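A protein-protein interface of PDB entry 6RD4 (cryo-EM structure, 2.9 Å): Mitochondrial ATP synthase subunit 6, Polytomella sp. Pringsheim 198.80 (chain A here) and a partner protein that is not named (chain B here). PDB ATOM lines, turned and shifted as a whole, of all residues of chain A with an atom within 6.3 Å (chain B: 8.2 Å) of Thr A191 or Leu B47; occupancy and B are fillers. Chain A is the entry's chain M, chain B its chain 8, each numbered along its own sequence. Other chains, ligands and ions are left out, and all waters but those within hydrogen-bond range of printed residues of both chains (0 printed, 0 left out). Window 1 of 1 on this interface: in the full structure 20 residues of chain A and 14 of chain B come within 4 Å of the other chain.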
ATOM      1  N   TRP A 151     -26.155 -33.432 -32.495  1.00  0.00           N
ATOM      2  CA  TRP A 151     -26.256 -33.906 -31.124  1.00  0.00           C
ATOM      3  C   TRP A 151     -27.264 -35.022 -30.996  1.00  0.00           C
ATOM      4  O   TRP A 151     -27.049 -35.954 -30.232  1.00  0.00           O
ATOM      5  CB  TRP A 151     -26.660 -32.788 -30.191  1.00  0.00           C
ATOM      6  CG  TRP A 151     -25.745 -31.678 -30.127  1.00  0.00           C
ATOM      7  CD1 TRP A 151     -24.464 -31.654 -30.526  1.00  0.00           C
ATOM      8  CD2 TRP A 151     -26.037 -30.391 -29.625  1.00  0.00           C
ATOM      9  NE1 TRP A 151     -23.929 -30.429 -30.302  1.00  0.00           N
ATOM     10  CE2 TRP A 151     -24.880 -29.635 -29.734  1.00  0.00           C
ATOM     11  CE3 TRP A 151     -27.166 -29.810 -29.071  1.00  0.00           C
ATOM     12  CZ2 TRP A 151     -24.824 -28.333 -29.340  1.00  0.00           C
ATOM     13  CZ3 TRP A 151     -27.104 -28.528 -28.684  1.00  0.00           C
ATOM     14  CH2 TRP A 151     -25.950 -27.797 -28.811  1.00  0.00           C
ATOM     15  N   THR A 154     -25.819 -38.110 -32.280  1.00  0.00           N
ATOM     16  CA  THR A 154     -24.832 -38.587 -31.332  1.00  0.00           C
ATOM     17  C   THR A 154     -25.504 -39.386 -30.239  1.00  0.00           C
ATOM     18  O   THR A 154     -25.037 -40.459 -29.872  1.00  0.00           O
ATOM     19  CB  THR A 154     -24.080 -37.401 -30.759  1.00  0.00           C
ATOM     20  OG1 THR A 154     -23.326 -36.802 -31.800  1.00  0.00           O
ATOM     21  CG2 THR A 154     -23.182 -37.793 -29.670  1.00  0.00           C
ATOM     22  N   PHE A 155     -26.629 -38.897 -29.737  1.00  0.00           N
ATOM     23  CA  PHE A 155     -27.351 -39.598 -28.691  1.00  0.00           C
ATOM     24  C   PHE A 155     -28.200 -40.719 -29.238  1.00  0.00           C
ATOM     25  O   PHE A 155     -28.562 -41.616 -28.497  1.00  0.00           O
ATOM     26  CB  PHE A 155     -28.222 -38.623 -27.931  1.00  0.00           C
ATOM     27  CG  PHE A 155     -27.456 -37.741 -27.036  1.00  0.00           C
ATOM     28  CD1 PHE A 155     -26.704 -38.272 -26.028  1.00  0.00           C
ATOM     29  CD2 PHE A 155     -27.480 -36.388 -27.198  1.00  0.00           C
ATOM     30  CE1 PHE A 155     -25.996 -37.471 -25.205  1.00  0.00           C
ATOM     31  CE2 PHE A 155     -26.757 -35.583 -26.380  1.00  0.00           C
ATOM     32  CZ  PHE A 155     -26.020 -36.128 -25.380  1.00  0.00           C
ATOM     33  N   VAL A 186     -29.175 -36.038 -17.841  1.00  0.00           N
ATOM     34  CA  VAL A 186     -28.845 -34.745 -17.262  1.00  0.00           C
ATOM     35  C   VAL A 186     -28.004 -33.937 -18.237  1.00  0.00           C
ATOM     36  O   VAL A 186     -28.112 -32.712 -18.302  1.00  0.00           O
ATOM     37  CB  VAL A 186     -28.146 -34.956 -15.908  1.00  0.00           C
ATOM     38  CG1 VAL A 186     -27.726 -33.671 -15.290  1.00  0.00           C
ATOM     39  CG2 VAL A 186     -29.072 -35.640 -14.970  1.00  0.00           C
ATOM     40  N   SER A 187     -27.206 -34.605 -19.053  1.00  0.00           N
ATOM     41  CA  SER A 187     -26.311 -33.914 -19.959  1.00  0.00           C
ATOM     42  C   SER A 187     -27.037 -33.324 -21.149  1.00  0.00           C
ATOM     43  O   SER A 187     -26.562 -32.358 -21.741  1.00  0.00           O
ATOM     44  CB  SER A 187     -25.262 -34.879 -20.426  1.00  0.00           C
ATOM     45  OG  SER A 187     -24.510 -35.303 -19.323  1.00  0.00           O
ATOM     46  N   VAL A 188     -28.149 -33.921 -21.552  1.00  0.00           N
ATOM     47  CA  VAL A 188     -29.029 -33.292 -22.520  1.00  0.00           C
ATOM     48  C   VAL A 188     -29.756 -32.123 -21.894  1.00  0.00           C
ATOM     49  O   VAL A 188     -29.918 -31.070 -22.516  1.00  0.00           O
ATOM     50  CB  VAL A 188     -30.009 -34.330 -23.064  1.00  0.00           C
ATOM     51  CG1 VAL A 188     -30.941 -33.708 -23.998  1.00  0.00           C
ATOM     52  CG2 VAL A 188     -29.258 -35.330 -23.785  1.00  0.00           C
ATOM     53  N   TRP A 189     -30.207 -32.283 -20.661  1.00  0.00           N
ATOM     54  CA  TRP A 189     -30.929 -31.214 -19.999  1.00  0.00           C
ATOM     55  C   TRP A 189     -30.019 -30.042 -19.695  1.00  0.00           C
ATOM     56  O   TRP A 189     -30.458 -28.895 -19.704  1.00  0.00           O
ATOM     57  CB  TRP A 189     -31.565 -31.743 -18.728  1.00  0.00           C
ATOM     58  CG  TRP A 189     -32.188 -30.698 -17.888  1.00  0.00           C
ATOM     59  CD1 TRP A 189     -33.458 -30.261 -17.957  1.00  0.00           C
ATOM     60  CD2 TRP A 189     -31.568 -29.968 -16.836  1.00  0.00           C
ATOM     61  NE1 TRP A 189     -33.673 -29.296 -17.026  1.00  0.00           N
ATOM     62  CE2 TRP A 189     -32.519 -29.097 -16.325  1.00  0.00           C
ATOM     63  CE3 TRP A 189     -30.291 -29.960 -16.291  1.00  0.00           C
ATOM     64  CZ2 TRP A 189     -32.240 -28.235 -15.302  1.00  0.00           C
ATOM     65  CZ3 TRP A 189     -30.019 -29.103 -15.288  1.00  0.00           C
ATOM     66  CH2 TRP A 189     -30.981 -28.257 -14.798  1.00  0.00           C
ATOM     67  N   ALA A 190     -28.760 -30.304 -19.392  1.00  0.00           N
ATOM     68  CA  ALA A 190     -27.858 -29.202 -19.136  1.00  0.00           C
ATOM     69  C   ALA A 190     -27.436 -28.530 -20.419  1.00  0.00           C
ATOM     70  O   ALA A 190     -27.175 -27.334 -20.421  1.00  0.00           O
ATOM     71  CB  ALA A 190     -26.651 -29.691 -18.366  1.00  0.00           C
ATOM     72  N   THR A 191     -27.373 -29.272 -21.517  1.00  0.00           N
ATOM     73  CA  THR A 191     -27.065 -28.696 -22.815  1.00  0.00           C
ATOM     74  C   THR A 191     -28.177 -27.786 -23.285  1.00  0.00           C
ATOM     75  O   THR A 191     -27.916 -26.749 -23.895  1.00  0.00           O
ATOM     76  CB  THR A 191     -26.857 -29.820 -23.803  1.00  0.00           C
ATOM     77  OG1 THR A 191     -25.912 -30.731 -23.257  1.00  0.00           O
ATOM     78  CG2 THR A 191     -26.363 -29.323 -25.096  1.00  0.00           C
ATOM     79  N   ALA A 192     -29.420 -28.159 -23.013  1.00  0.00           N
ATOM     80  CA  ALA A 192     -30.530 -27.285 -23.327  1.00  0.00           C
ATOM     81  C   ALA A 192     -30.501 -26.040 -22.471  1.00  0.00           C
ATOM     82  O   ALA A 192     -30.750 -24.948 -22.968  1.00  0.00           O
ATOM     83  CB  ALA A 192     -31.837 -28.029 -23.131  1.00  0.00           C
ATOM     84  N   THR A 193     -30.143 -26.176 -21.202  1.00  0.00           N
ATOM     85  CA  THR A 193     -30.137 -25.040 -20.297  1.00  0.00           C
ATOM     86  C   THR A 193     -28.971 -24.104 -20.569  1.00  0.00           C
ATOM     87  O   THR A 193     -29.146 -22.887 -20.557  1.00  0.00           O
ATOM     88  CB  THR A 193     -30.124 -25.555 -18.874  1.00  0.00           C
ATOM     89  OG1 THR A 193     -31.236 -26.430 -18.717  1.00  0.00           O
ATOM     90  CG2 THR A 193     -30.272 -24.446 -17.900  1.00  0.00           C
ATOM     91  N   ILE A 194     -27.785 -24.646 -20.847  1.00  0.00           N
ATOM     92  CA  ILE A 194     -26.632 -23.825 -21.207  1.00  0.00           C
ATOM     93  C   ILE A 194     -26.879 -23.099 -22.516  1.00  0.00           C
ATOM     94  O   ILE A 194     -26.474 -21.947 -22.682  1.00  0.00           O
ATOM     95  CB  ILE A 194     -25.378 -24.711 -21.255  1.00  0.00           C
ATOM     96  CG1 ILE A 194     -24.958 -25.068 -19.853  1.00  0.00           C
ATOM     97  CG2 ILE A 194     -24.224 -24.012 -21.841  1.00  0.00           C
ATOM     98  CD1 ILE A 194     -23.891 -26.046 -19.802  1.00  0.00           C
ATOM     99  N   LEU A 195     -27.598 -23.723 -23.441  1.00  0.00           N
ATOM    100  CA  LEU A 195     -28.007 -23.028 -24.649  1.00  0.00           C
ATOM    101  C   LEU A 195     -29.012 -21.931 -24.344  1.00  0.00           C
ATOM    102  O   LEU A 195     -28.904 -20.826 -24.871  1.00  0.00           O
ATOM    103  CB  LEU A 195     -28.586 -24.025 -25.641  1.00  0.00           C
ATOM    104  CG  LEU A 195     -29.147 -23.515 -26.949  1.00  0.00           C
ATOM    105  CD1 LEU A 195     -28.071 -23.304 -27.919  1.00  0.00           C
ATOM    106  CD2 LEU A 195     -30.060 -24.532 -27.464  1.00  0.00           C
ATOM    107  N   GLY A 196     -29.984 -22.202 -23.481  1.00  0.00           N
ATOM    108  CA  GLY A 196     -30.956 -21.186 -23.135  1.00  0.00           C
ATOM    109  C   GLY A 196     -30.440 -20.109 -22.216  1.00  0.00           C
ATOM    110  O   GLY A 196     -31.000 -19.014 -22.189  1.00  0.00           O
ATOM    111  N   VAL A 307     -33.868 -29.127 -26.449  1.00  0.00           N
ATOM    112  CA  VAL A 307     -32.847 -28.218 -26.942  1.00  0.00           C
ATOM    113  C   VAL A 307     -33.432 -27.288 -27.983  1.00  0.00           C
ATOM    114  O   VAL A 307     -33.040 -26.125 -28.079  1.00  0.00           O
ATOM    115  CB  VAL A 307     -31.647 -29.023 -27.473  1.00  0.00           C
ATOM    116  CG1 VAL A 307     -30.585 -28.147 -27.963  1.00  0.00           C
ATOM    117  CG2 VAL A 307     -31.070 -29.861 -26.372  1.00  0.00           C
ATOM    118  N   PHE A 310     -34.913 -23.530 -26.992  1.00  0.00           N
ATOM    119  CA  PHE A 310     -34.058 -22.360 -26.955  1.00  0.00           C
ATOM    120  C   PHE A 310     -33.296 -22.159 -28.244  1.00  0.00           C
ATOM    121  O   PHE A 310     -32.271 -21.480 -28.251  1.00  0.00           O
ATOM    122  CB  PHE A 310     -33.095 -22.469 -25.788  1.00  0.00           C
ATOM    123  CG  PHE A 310     -33.737 -22.956 -24.550  1.00  0.00           C
ATOM    124  CD1 PHE A 310     -34.558 -22.133 -23.826  1.00  0.00           C
ATOM    125  CD2 PHE A 310     -33.541 -24.239 -24.117  1.00  0.00           C
ATOM    126  CE1 PHE A 310     -35.168 -22.583 -22.702  1.00  0.00           C
ATOM    127  CE2 PHE A 310     -34.135 -24.687 -22.975  1.00  0.00           C
ATOM    128  CZ  PHE A 310     -34.948 -23.859 -22.270  1.00  0.00           C
ATOM    129  N   LEU B  40     -15.555 -27.997 -32.573  1.00  0.00           N
ATOM    130  CA  LEU B  40     -15.923 -28.562 -31.287  1.00  0.00           C
ATOM    131  C   LEU B  40     -16.209 -27.484 -30.263  1.00  0.00           C
ATOM    132  O   LEU B  40     -17.176 -27.578 -29.512  1.00  0.00           O
ATOM    133  CB  LEU B  40     -14.827 -29.486 -30.797  1.00  0.00           C
ATOM    134  CG  LEU B  40     -14.915 -30.084 -29.418  1.00  0.00           C
ATOM    135  CD1 LEU B  40     -16.127 -30.937 -29.318  1.00  0.00           C
ATOM    136  CD2 LEU B  40     -13.698 -30.899 -29.194  1.00  0.00           C
ATOM    137  N   ILE B  41     -15.394 -26.448 -30.218  1.00  0.00           N
ATOM    138  CA  ILE B  41     -15.614 -25.377 -29.257  1.00  0.00           C
ATOM    139  C   ILE B  41     -16.619 -24.331 -29.744  1.00  0.00           C
ATOM    140  O   ILE B  41     -17.471 -23.948 -28.943  1.00  0.00           O
ATOM    141  CB  ILE B  41     -14.267 -24.784 -28.823  1.00  0.00           C
ATOM    142  CG1 ILE B  41     -13.541 -25.828 -27.989  1.00  0.00           C
ATOM    143  CG2 ILE B  41     -14.430 -23.539 -28.033  1.00  0.00           C
ATOM    144  CD1 ILE B  41     -12.132 -25.532 -27.764  1.00  0.00           C
ATOM    145  N   ARG B  43     -19.205 -24.763 -31.830  1.00  0.00           N
ATOM    146  CA  ARG B  43     -20.516 -25.333 -32.072  1.00  0.00           C
ATOM    147  C   ARG B  43     -20.996 -26.272 -30.994  1.00  0.00           C
ATOM    148  O   ARG B  43     -22.191 -26.306 -30.735  1.00  0.00           O
ATOM    149  CB  ARG B  43     -20.541 -26.092 -33.398  1.00  0.00           C
ATOM    150  CG  ARG B  43     -20.197 -25.282 -34.571  1.00  0.00           C
ATOM    151  CD  ARG B  43     -21.288 -24.303 -34.842  1.00  0.00           C
ATOM    152  NE  ARG B  43     -22.439 -24.921 -35.461  1.00  0.00           N
ATOM    153  CZ  ARG B  43     -23.654 -24.409 -35.416  1.00  0.00           C
ATOM    154  NH1 ARG B  43     -23.851 -23.289 -34.769  1.00  0.00           N
ATOM    155  NH2 ARG B  43     -24.659 -25.012 -36.011  1.00  0.00           N
ATOM    156  N   HIS B  44     -20.112 -27.056 -30.389  1.00  0.00           N
ATOM    157  CA  HIS B  44     -20.517 -28.079 -29.445  1.00  0.00           C
ATOM    158  C   HIS B  44     -20.084 -27.777 -28.029  1.00  0.00           C
ATOM    159  O   HIS B  44     -19.944 -28.703 -27.246  1.00  0.00           O
ATOM    160  CB  HIS B  44     -19.951 -29.445 -29.820  1.00  0.00           C
ATOM    161  CG  HIS B  44     -20.183 -29.848 -31.237  1.00  0.00           C
ATOM    162  ND1 HIS B  44     -21.403 -29.748 -31.855  1.00  0.00           N
ATOM    163  CD2 HIS B  44     -19.347 -30.386 -32.143  1.00  0.00           C
ATOM    164  CE1 HIS B  44     -21.301 -30.177 -33.095  1.00  0.00           C
ATOM    165  NE2 HIS B  44     -20.062 -30.573 -33.293  1.00  0.00           N
ATOM    166  N   TRP B  45     -19.844 -26.524 -27.673  1.00  0.00           N
ATOM    167  CA  TRP B  45     -19.482 -26.259 -26.289  1.00  0.00           C
ATOM    168  C   TRP B  45     -20.671 -26.343 -25.354  1.00  0.00           C
ATOM    169  O   TRP B  45     -20.479 -26.413 -24.143  1.00  0.00           O
ATOM    170  CB  TRP B  45     -18.817 -24.897 -26.150  1.00  0.00           C
ATOM    171  CG  TRP B  45     -19.715 -23.738 -26.276  1.00  0.00           C
ATOM    172  CD1 TRP B  45     -20.036 -23.088 -27.403  1.00  0.00           C
ATOM    173  CD2 TRP B  45     -20.394 -23.065 -25.219  1.00  0.00           C
ATOM    174  NE1 TRP B  45     -20.884 -22.059 -27.133  1.00  0.00           N
ATOM    175  CE2 TRP B  45     -21.128 -22.036 -25.791  1.00  0.00           C
ATOM    176  CE3 TRP B  45     -20.469 -23.256 -23.843  1.00  0.00           C
ATOM    177  CZ2 TRP B  45     -21.912 -21.195 -25.043  1.00  0.00           C
ATOM    178  CZ3 TRP B  45     -21.244 -22.432 -23.117  1.00  0.00           C
ATOM    179  CH2 TRP B  45     -21.957 -21.415 -23.710  1.00  0.00           C
ATOM    180  N   TYR B  46     -21.886 -26.330 -25.883  1.00  0.00           N
ATOM    181  CA  TYR B  46     -23.054 -26.579 -25.063  1.00  0.00           C
ATOM    182  C   TYR B  46     -23.103 -28.025 -24.609  1.00  0.00           C
ATOM    183  O   TYR B  46     -23.514 -28.300 -23.486  1.00  0.00           O
ATOM    184  CB  TYR B  46     -24.311 -26.244 -25.836  1.00  0.00           C
ATOM    185  CG  TYR B  46     -24.258 -24.968 -26.604  1.00  0.00           C
ATOM    186  CD1 TYR B  46     -24.604 -23.782 -26.015  1.00  0.00           C
ATOM    187  CD2 TYR B  46     -23.901 -24.958 -27.928  1.00  0.00           C
ATOM    188  CE1 TYR B  46     -24.578 -22.626 -26.715  1.00  0.00           C
ATOM    189  CE2 TYR B  46     -23.862 -23.811 -28.629  1.00  0.00           C
ATOM    190  CZ  TYR B  46     -24.198 -22.649 -28.020  1.00  0.00           C
ATOM    191  OH  TYR B  46     -24.159 -21.489 -28.742  1.00  0.00           O
ATOM    192  N   LEU B  47     -22.708 -28.967 -25.465  1.00  0.00           N
ATOM    193  CA  LEU B  47     -22.641 -30.359 -25.032  1.00  0.00           C
ATOM    194  C   LEU B  47     -21.513 -30.589 -24.061  1.00  0.00           C
ATOM    195  O   LEU B  47     -21.672 -31.338 -23.100  1.00  0.00           O
ATOM    196  CB  LEU B  47     -22.441 -31.309 -26.192  1.00  0.00           C
ATOM    197  CG  LEU B  47     -23.601 -32.021 -26.818  1.00  0.00           C
ATOM    198  CD1 LEU B  47     -23.016 -33.106 -27.631  1.00  0.00           C
ATOM    199  CD2 LEU B  47     -24.464 -32.595 -25.754  1.00  0.00           C
ATOM    200  N   LEU B  48     -20.353 -30.009 -24.322  1.00  0.00           N
ATOM    201  CA  LEU B  48     -19.227 -30.206 -23.429  1.00  0.00           C
ATOM    202  C   LEU B  48     -19.453 -29.518 -22.102  1.00  0.00           C
ATOM    203  O   LEU B  48     -18.903 -29.940 -21.091  1.00  0.00           O
ATOM    204  CB  LEU B  48     -17.958 -29.679 -24.065  1.00  0.00           C
ATOM    205  CG  LEU B  48     -17.550 -30.214 -25.422  1.00  0.00           C
ATOM    206  CD1 LEU B  48     -16.181 -29.685 -25.695  1.00  0.00           C
ATOM    207  CD2 LEU B  48     -17.572 -31.710 -25.448  1.00  0.00           C
ATOM    208  N   GLY B  49     -20.243 -28.454 -22.087  1.00  0.00           N
ATOM    209  CA  GLY B  49     -20.669 -27.890 -20.829  1.00  0.00           C
ATOM    210  C   GLY B  49     -21.699 -28.741 -20.138  1.00  0.00           C
ATOM    211  O   GLY B  49     -21.752 -28.766 -18.912  1.00  0.00           O
ATOM    212  N   GLY B  50     -22.534 -29.438 -20.895  1.00  0.00           N
ATOM    213  CA  GLY B  50     -23.518 -30.304 -20.286  1.00  0.00           C
ATOM    214  C   GLY B  50     -22.937 -31.599 -19.775  1.00  0.00           C
ATOM    215  O   GLY B  50     -23.441 -32.163 -18.810  1.00  0.00           O
ATOM    216  N   PHE B  51     -21.897 -32.110 -20.428  1.00  0.00           N
ATOM    217  CA  PHE B  51     -21.183 -33.254 -19.886  1.00  0.00           C
ATOM    218  C   PHE B  51     -20.348 -32.859 -18.685  1.00  0.00           C
ATOM    219  O   PHE B  51     -20.099 -33.682 -17.814  1.00  0.00           O
ATOM    220  CB  PHE B  51     -20.281 -33.879 -20.944  1.00  0.00           C
ATOM    221  CG  PHE B  51     -21.010 -34.621 -22.011  1.00  0.00           C
ATOM    222  CD1 PHE B  51     -22.056 -35.445 -21.700  1.00  0.00           C
ATOM    223  CD2 PHE B  51     -20.623 -34.517 -23.323  1.00  0.00           C
ATOM    224  CE1 PHE B  51     -22.730 -36.126 -22.668  1.00  0.00           C
ATOM    225  CE2 PHE B  51     -21.284 -35.206 -24.294  1.00  0.00           C
ATOM    226  CZ  PHE B  51     -22.345 -36.004 -23.961  1.00  0.00           C
ATOM    227  N   THR B  52     -19.890 -31.612 -18.632  1.00  0.00           N
ATOM    228  CA  THR B  52     -19.124 -31.141 -17.486  1.00  0.00           C
ATOM    229  C   THR B  52     -20.022 -30.926 -16.285  1.00  0.00           C
ATOM    230  O   THR B  52     -19.618 -31.188 -15.150  1.00  0.00           O
ATOM    231  CB  THR B  52     -18.395 -29.854 -17.851  1.00  0.00           C
ATOM    232  OG1 THR B  52     -17.527 -30.119 -18.950  1.00  0.00           O
ATOM    233  CG2 THR B  52     -17.551 -29.344 -16.728  1.00  0.00           C
ATOM    234  N   PHE B  53     -21.250 -30.471 -16.512  1.00  0.00           N
ATOM    235  CA  PHE B  53     -22.185 -30.286 -15.415  1.00  0.00           C
ATOM    236  C   PHE B  53     -22.560 -31.606 -14.770  1.00  0.00           C
ATOM    237  O   PHE B  53     -22.701 -31.682 -13.553  1.00  0.00           O
ATOM    238  CB  PHE B  53     -23.434 -29.578 -15.905  1.00  0.00           C
ATOM    239  CG  PHE B  53     -24.478 -29.424 -14.858  1.00  0.00           C
ATOM    240  CD1 PHE B  53     -24.341 -28.478 -13.879  1.00  0.00           C
ATOM    241  CD2 PHE B  53     -25.604 -30.216 -14.857  1.00  0.00           C
ATOM    242  CE1 PHE B  53     -25.293 -28.331 -12.923  1.00  0.00           C
ATOM    243  CE2 PHE B  53     -26.549 -30.075 -13.896  1.00  0.00           C
ATOM    244  CZ  PHE B  53     -26.395 -29.131 -12.934  1.00  0.00           C
ATOM    245  N   THR B  54     -22.714 -32.656 -15.558  1.00  0.00           N
ATOM    246  CA  THR B  54     -23.123 -33.935 -15.008  1.00  0.00           C
ATOM    247  C   THR B  54     -22.007 -34.601 -14.230  1.00  0.00           C
ATOM    248  O   THR B  54     -22.260 -35.181 -13.178  1.00  0.00           O
ATOM    249  CB  THR B  54     -23.589 -34.831 -16.132  1.00  0.00           C
ATOM    250  OG1 THR B  54     -24.635 -34.167 -16.824  1.00  0.00           O
ATOM    251  CG2 THR B  54     -24.124 -36.103 -15.618  1.00  0.00           C
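The side-chain hydroxyl (OG) of Ser A187 sits at hydrogen-bond distance from the side-chain hydroxyl (OG1) of Thr B54 (2.7 Å). The indole nitrogen (NE1) of Trp A151 lies within hydrogen-bond range of a ring nitrogen (ND1) of His B44, at 3.0 Å. OG of Ser A187 is in hydrogen-bond range of O of Gly B50 (3.4 Å). The side-chain hydroxyl (OG1) of Thr A191 lies within hydrogen-bond range of the backbone carbonyl oxygen (O) of Tyr B46 (3.4 Å).
The backbone carbonyl oxygen of Leu B40 is in hydrogen-bond range of the backbone NH of Trp B45 (3.4 Å). The backbone carbonyl oxygen of Trp A189 is in hydrogen-bond range of the side-chain hydroxyl of Thr A193, 2.8 Å away. The backbone carbonyl oxygen (O) of Gly B50 sits at hydrogen-bond distance from the side-chain hydroxyl (OG1) of Thr B54 (3.1 Å).
CH2 of Trp A151 touches CD2 of Tyr B46, 3.6 Å away. Leu B47 touches Phe A155. Phe A155 touches Phe B51 (CZ to CZ, 3.9 Å). Val A186 touches Thr B54. OG of Ser A187 touches CD1 of Phe B51, at 3.4 Å. Trp A189 touches Phe B53. Gly B50 touches Ala A190. OG1 of Thr A191 touches CD2 of Leu B47 (3.4 Å). Thr A191 touches Gly B50. C of Gly B49 touches CD1 of Ile A194, at 3.5 Å.
Thr A154 touches none of the printed residues of chain B. Thr A191 touches just these residues of chain B: Tyr B46, Leu B47 and Gly B50. No residue of chain B comes within 4 Å of Ala A192. Ile B41 touches none of the printed residues of chain A. Of the printed residues of chain A, Arg B43 touches Trp A151 (3.6 Å). Of the printed residues of chain A, His B44 touches Trp A151. Leu B47 touches three residues of chain A. Printed residues of chain A within 4 Å of Phe B53: Trp A189 (3.9 Å) and Ala A190 (3.7 Å). The nearest printed residue of chain A that does not touch Thr B54 is Ala A190 (5.1 Å).
Printed residues of chain A that touch a printed residue of chain B: Trp A151, Phe A155, Val A186, Ser A187, Trp A189, Ala A190, Thr A191, Ile A194 and Leu A195. Of the 14 printed residues of chain B, 10 touch a printed residue of chain A. Hydrophobic or aromatic side chains of chain B within 4 Å of the printed part of chain A: His B44, Trp B45, Tyr B46, Leu B47, Phe B51 and Phe B53. Along chain B the printed residues that touch a printed residue of chain A span positions 43 to 54. Among the printed residues, no Asp or Glu carboxylate lies within 4 Å of a Lys or Arg side-chain nitrogen of the other chain.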
